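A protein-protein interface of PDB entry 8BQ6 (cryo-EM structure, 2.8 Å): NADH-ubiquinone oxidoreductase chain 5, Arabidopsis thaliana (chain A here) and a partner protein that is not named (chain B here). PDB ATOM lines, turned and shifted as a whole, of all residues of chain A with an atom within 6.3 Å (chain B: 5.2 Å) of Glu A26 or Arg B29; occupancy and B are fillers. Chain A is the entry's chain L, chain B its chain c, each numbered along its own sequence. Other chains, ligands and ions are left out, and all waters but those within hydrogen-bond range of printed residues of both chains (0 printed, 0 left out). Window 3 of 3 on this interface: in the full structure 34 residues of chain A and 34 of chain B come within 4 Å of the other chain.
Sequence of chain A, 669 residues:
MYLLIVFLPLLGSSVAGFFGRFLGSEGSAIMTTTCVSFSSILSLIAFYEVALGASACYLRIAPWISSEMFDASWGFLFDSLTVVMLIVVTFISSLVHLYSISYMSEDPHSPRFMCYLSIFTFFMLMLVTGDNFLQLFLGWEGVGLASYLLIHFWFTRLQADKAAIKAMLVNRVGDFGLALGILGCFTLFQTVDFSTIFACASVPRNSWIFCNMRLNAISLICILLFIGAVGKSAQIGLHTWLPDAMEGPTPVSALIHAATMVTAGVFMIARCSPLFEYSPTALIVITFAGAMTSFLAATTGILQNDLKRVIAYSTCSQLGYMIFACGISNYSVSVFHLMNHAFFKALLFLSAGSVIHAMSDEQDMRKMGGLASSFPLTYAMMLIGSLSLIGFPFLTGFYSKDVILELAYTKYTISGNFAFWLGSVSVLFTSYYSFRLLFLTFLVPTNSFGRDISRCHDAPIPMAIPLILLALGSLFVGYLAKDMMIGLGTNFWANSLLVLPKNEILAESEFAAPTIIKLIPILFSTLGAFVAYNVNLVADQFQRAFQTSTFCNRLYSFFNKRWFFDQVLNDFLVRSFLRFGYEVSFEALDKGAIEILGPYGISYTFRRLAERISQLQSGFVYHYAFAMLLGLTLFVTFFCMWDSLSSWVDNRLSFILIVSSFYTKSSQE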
ATOM      1  N   LEU A  23     -24.765  -9.862  -4.225  1.00  0.00           N
ATOM      2  CA  LEU A  23     -25.097  -8.446  -4.184  1.00  0.00           C
ATOM      3  C   LEU A  23     -23.884  -7.557  -3.966  1.00  0.00           C
ATOM      4  O   LEU A  23     -23.870  -6.419  -4.445  1.00  0.00           O
ATOM      5  CB  LEU A  23     -26.110  -8.181  -3.065  1.00  0.00           C
ATOM      6  CG  LEU A  23     -27.500  -8.824  -3.140  1.00  0.00           C
ATOM      7  CD1 LEU A  23     -28.545  -7.934  -2.488  1.00  0.00           C
ATOM      8  CD2 LEU A  23     -27.898  -9.139  -4.566  1.00  0.00           C
ATOM      9  N   GLY A  24     -22.876  -8.041  -3.249  1.00  0.00           N
ATOM     10  CA  GLY A  24     -21.724  -7.214  -2.970  1.00  0.00           C
ATOM     11  C   GLY A  24     -22.026  -6.129  -1.946  1.00  0.00           C
ATOM     12  O   GLY A  24     -23.065  -6.105  -1.297  1.00  0.00           O
ATOM     13  N   SER A  25     -21.064  -5.211  -1.825  1.00  0.00           N
ATOM     14  CA  SER A  25     -21.186  -4.119  -0.862  1.00  0.00           C
ATOM     15  C   SER A  25     -22.364  -3.213  -1.194  1.00  0.00           C
ATOM     16  O   SER A  25     -23.095  -2.771  -0.300  1.00  0.00           O
ATOM     17  CB  SER A  25     -19.894  -3.303  -0.826  1.00  0.00           C
ATOM     18  OG  SER A  25     -18.808  -4.074  -0.354  1.00  0.00           O
ATOM     19  N   GLU A  26     -22.545  -2.901  -2.477  1.00  0.00           N
ATOM     20  CA  GLU A  26     -23.578  -1.953  -2.881  1.00  0.00           C
ATOM     21  C   GLU A  26     -24.961  -2.591  -2.849  1.00  0.00           C
ATOM     22  O   GLU A  26     -25.940  -1.962  -2.432  1.00  0.00           O
ATOM     23  CB  GLU A  26     -23.266  -1.422  -4.275  1.00  0.00           C
ATOM     24  CG  GLU A  26     -22.142  -0.414  -4.310  1.00  0.00           C
ATOM     25  CD  GLU A  26     -20.794  -1.060  -4.508  1.00  0.00           C
ATOM     26  OE1 GLU A  26     -20.603  -1.727  -5.545  1.00  0.00           O
ATOM     27  OE2 GLU A  26     -19.918  -0.887  -3.636  1.00  0.00           O
ATOM     28  N   GLY A  27     -25.063  -3.838  -3.311  1.00  0.00           N
ATOM     29  CA  GLY A  27     -26.354  -4.507  -3.322  1.00  0.00           C
ATOM     30  C   GLY A  27     -26.882  -4.791  -1.932  1.00  0.00           C
ATOM     31  O   GLY A  27     -28.064  -4.589  -1.647  1.00  0.00           O
ATOM     32  N   SER A  28     -26.013  -5.281  -1.044  1.00  0.00           N
ATOM     33  CA  SER A  28     -26.442  -5.568   0.319  1.00  0.00           C
ATOM     34  C   SER A  28     -26.784  -4.296   1.081  1.00  0.00           C
ATOM     35  O   SER A  28     -27.644  -4.319   1.969  1.00  0.00           O
ATOM     36  CB  SER A  28     -25.361  -6.358   1.057  1.00  0.00           C
ATOM     37  OG  SER A  28     -25.110  -7.592   0.410  1.00  0.00           O
ATOM     38  N   ALA A  29     -26.118  -3.185   0.762  1.00  0.00           N
ATOM     39  CA  ALA A  29     -26.442  -1.913   1.400  1.00  0.00           C
ATOM     40  C   ALA A  29     -27.841  -1.443   1.018  1.00  0.00           C
ATOM     41  O   ALA A  29     -28.590  -0.935   1.860  1.00  0.00           O
ATOM     42  CB  ALA A  29     -25.397  -0.862   1.027  1.00  0.00           C
ATOM     43  N   ILE A  30     -28.205  -1.586  -0.256  1.00  0.00           N
ATOM     44  CA  ILE A  30     -29.529  -1.161  -0.702  1.00  0.00           C
ATOM     45  C   ILE A  30     -30.599  -2.089  -0.149  1.00  0.00           C
ATOM     46  O   ILE A  30     -31.688  -1.651   0.240  1.00  0.00           O
ATOM     47  CB  ILE A  30     -29.578  -1.089  -2.239  1.00  0.00           C
ATOM     48  CG1 ILE A  30     -29.266   0.324  -2.698  1.00  0.00           C
ATOM     49  CG2 ILE A  30     -30.931  -1.473  -2.762  1.00  0.00           C
ATOM     50  CD1 ILE A  30     -27.862   0.693  -2.466  1.00  0.00           C
ATOM     51  N   MET A  31     -30.305  -3.388  -0.113  1.00  0.00           N
ATOM     52  CA  MET A  31     -31.309  -4.367   0.283  1.00  0.00           C
ATOM     53  C   MET A  31     -31.726  -4.171   1.734  1.00  0.00           C
ATOM     54  O   MET A  31     -32.920  -4.144   2.051  1.00  0.00           O
ATOM     55  CB  MET A  31     -30.768  -5.779   0.070  1.00  0.00           C
ATOM     56  CG  MET A  31     -31.541  -6.600  -0.941  1.00  0.00           C
ATOM     57  SD  MET A  31     -33.271  -6.819  -0.499  1.00  0.00           S
ATOM     58  CE  MET A  31     -33.120  -7.575   1.112  1.00  0.00           C
ATOM     59  N   PRO A 111     -21.079  -6.053   3.795  1.00  0.00           N
ATOM     60  CA  PRO A 111     -22.330  -6.835   3.746  1.00  0.00           C
ATOM     61  C   PRO A 111     -22.646  -7.580   5.031  1.00  0.00           C
ATOM     62  O   PRO A 111     -23.821  -7.678   5.408  1.00  0.00           O
ATOM     63  CB  PRO A 111     -22.093  -7.796   2.574  1.00  0.00           C
ATOM     64  CG  PRO A 111     -21.095  -7.114   1.734  1.00  0.00           C
ATOM     65  CD  PRO A 111     -20.182  -6.423   2.685  1.00  0.00           C
ATOM     66  N   ASN B  27     -14.323  -7.054   0.214  1.00  0.00           N
ATOM     67  CA  ASN B  27     -14.399  -6.252  -1.010  1.00  0.00           C
ATOM     68  C   ASN B  27     -15.116  -7.012  -2.121  1.00  0.00           C
ATOM     69  O   ASN B  27     -14.626  -7.129  -3.246  1.00  0.00           O
ATOM     70  CB  ASN B  27     -13.010  -5.807  -1.469  1.00  0.00           C
ATOM     71  CG  ASN B  27     -12.292  -4.991  -0.429  1.00  0.00           C
ATOM     72  OD1 ASN B  27     -12.797  -3.967   0.028  1.00  0.00           O
ATOM     73  ND2 ASN B  27     -11.102  -5.437  -0.047  1.00  0.00           N
ATOM     74  N   CYS B  28     -16.291  -7.536  -1.793  1.00  0.00           N
ATOM     75  CA  CYS B  28     -17.082  -8.291  -2.753  1.00  0.00           C
ATOM     76  C   CYS B  28     -17.721  -7.320  -3.737  1.00  0.00           C
ATOM     77  O   CYS B  28     -18.500  -6.445  -3.341  1.00  0.00           O
ATOM     78  CB  CYS B  28     -18.132  -9.123  -2.021  1.00  0.00           C
ATOM     79  SG  CYS B  28     -19.048 -10.299  -3.027  1.00  0.00           S
ATOM     80  N   ARG B  29     -17.366  -7.455  -5.012  1.00  0.00           N
ATOM     81  CA  ARG B  29     -17.852  -6.587  -6.083  1.00  0.00           C
ATOM     82  C   ARG B  29     -18.327  -7.449  -7.243  1.00  0.00           C
ATOM     83  O   ARG B  29     -17.668  -7.516  -8.287  1.00  0.00           O
ATOM     84  CB  ARG B  29     -16.752  -5.637  -6.549  1.00  0.00           C
ATOM     85  CG  ARG B  29     -16.263  -4.669  -5.501  1.00  0.00           C
ATOM     86  CD  ARG B  29     -17.072  -3.404  -5.544  1.00  0.00           C
ATOM     87  NE  ARG B  29     -17.293  -2.968  -6.917  1.00  0.00           N
ATOM     88  CZ  ARG B  29     -17.838  -1.807  -7.250  1.00  0.00           C
ATOM     89  NH1 ARG B  29     -18.198  -0.926  -6.332  1.00  0.00           N
ATOM     90  NH2 ARG B  29     -18.026  -1.524  -8.535  1.00  0.00           N
ATOM     91  N   PRO B  30     -19.448  -8.149  -7.088  1.00  0.00           N
ATOM     92  CA  PRO B  30     -19.946  -8.965  -8.198  1.00  0.00           C
ATOM     93  C   PRO B  30     -20.277  -8.097  -9.404  1.00  0.00           C
ATOM     94  O   PRO B  30     -20.835  -7.006  -9.274  1.00  0.00           O
ATOM     95  CB  PRO B  30     -21.191  -9.644  -7.615  1.00  0.00           C
ATOM     96  CG  PRO B  30     -21.562  -8.835  -6.437  1.00  0.00           C
ATOM     97  CD  PRO B  30     -20.305  -8.248  -5.898  1.00  0.00           C
ATOM     98  N   LYS B  31     -19.915  -8.596 -10.588  1.00  0.00           N
ATOM     99  CA  LYS B  31     -20.025  -7.793 -11.804  1.00  0.00           C
ATOM    100  C   LYS B  31     -21.477  -7.477 -12.133  1.00  0.00           C
ATOM    101  O   LYS B  31     -21.802  -6.351 -12.528  1.00  0.00           O
ATOM    102  CB  LYS B  31     -19.346  -8.520 -12.966  1.00  0.00           C
ATOM    103  CG  LYS B  31     -19.741  -8.025 -14.347  1.00  0.00           C
ATOM    104  CD  LYS B  31     -18.931  -8.705 -15.450  1.00  0.00           C
ATOM    105  CE  LYS B  31     -18.403 -10.070 -15.020  1.00  0.00           C
ATOM    106  NZ  LYS B  31     -17.570 -10.722 -16.071  1.00  0.00           N
ATOM    107  N   TRP B  33     -23.994  -7.176 -10.079  1.00  0.00           N
ATOM    108  CA  TRP B  33     -24.623  -6.964  -8.781  1.00  0.00           C
ATOM    109  C   TRP B  33     -25.935  -6.201  -8.893  1.00  0.00           C
ATOM    110  O   TRP B  33     -26.756  -6.263  -7.973  1.00  0.00           O
ATOM    111  CB  TRP B  33     -23.660  -6.246  -7.827  1.00  0.00           C
ATOM    112  CG  TRP B  33     -23.427  -4.789  -8.102  1.00  0.00           C
ATOM    113  CD1 TRP B  33     -22.388  -4.248  -8.797  1.00  0.00           C
ATOM    114  CD2 TRP B  33     -24.232  -3.687  -7.662  1.00  0.00           C
ATOM    115  NE1 TRP B  33     -22.500  -2.881  -8.828  1.00  0.00           N
ATOM    116  CE2 TRP B  33     -23.624  -2.511  -8.139  1.00  0.00           C
ATOM    117  CE3 TRP B  33     -25.410  -3.581  -6.917  1.00  0.00           C
ATOM    118  CZ2 TRP B  33     -24.153  -1.246  -7.899  1.00  0.00           C
ATOM    119  CZ3 TRP B  33     -25.935  -2.323  -6.681  1.00  0.00           C
ATOM    120  CH2 TRP B  33     -25.306  -1.173  -7.169  1.00  0.00           C
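N of Ser A25 sits at hydrogen-bond distance from O of Cys B28 (3.2 Å).
The guanidinium group (NH1) of Arg B29 is in salt-bridge range of the side-chain carboxylate (OE1) of Glu A26, at 2.7 Å.
The backbone carbonyl oxygen (O) of Gly A24 lies within hydrogen-bond range of the side-chain hydroxyl (OG) of Ser A28 (3.1 Å).
Leu A23 touches Pro B30.
Leu A23 touches Trp B33.
CA of Gly A24 touches O of Cys B28, 3.3 Å away.
Gly A24 touches Pro B30.
Trp B33 touches Glu A26.
N of Gly A27 touches CE3 of Trp B33, at 3.6 Å.
Printed residues of chain B within 4 Å of Leu A23: Pro B30 (3.6 Å) and Trp B33 (3.4 Å).
Of the printed residues of chain B, Gly A24 touches Cys B28 (3.3 Å) and Pro B30 (3.4 Å).
Printed residues of chain B within 4 Å of Ser A25: Cys B28.
Glu A26 touches two residues of chain B.
Ser A28 touches none of the printed residues of chain B.
Of chain A, only Glu A26 (2.7 Å) comes within 4 Å of Arg B29.
Printed residues of chain A within 4 Å of Trp B33: Leu A23 (3.4 Å), Glu A26 (3.5 Å) and Gly A27 (3.6 Å).
The nearest printed residue of chain B that does not touch Glu A26 is Cys B28 (5.4 Å).
The nearest residue of chain A that does not touch Arg B29 is Gly A24 (4.8 Å).
Of the 6 printed residues of chain B, 4 touch a printed residue of chain A.
Printed residues of chain B that touch a printed residue of chain A: Cys B28, Arg B29, Pro B30 and Trp B33.
Hydrophobic or aromatic side chains of chain B within 4 Å of the printed part of chain A: Pro B30 and Trp B33.
Among the printed residues, Asp or Glu carboxylates within 4 Å of a Lys or Arg side-chain nitrogen of the other chain: Glu A26 with Arg B29.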
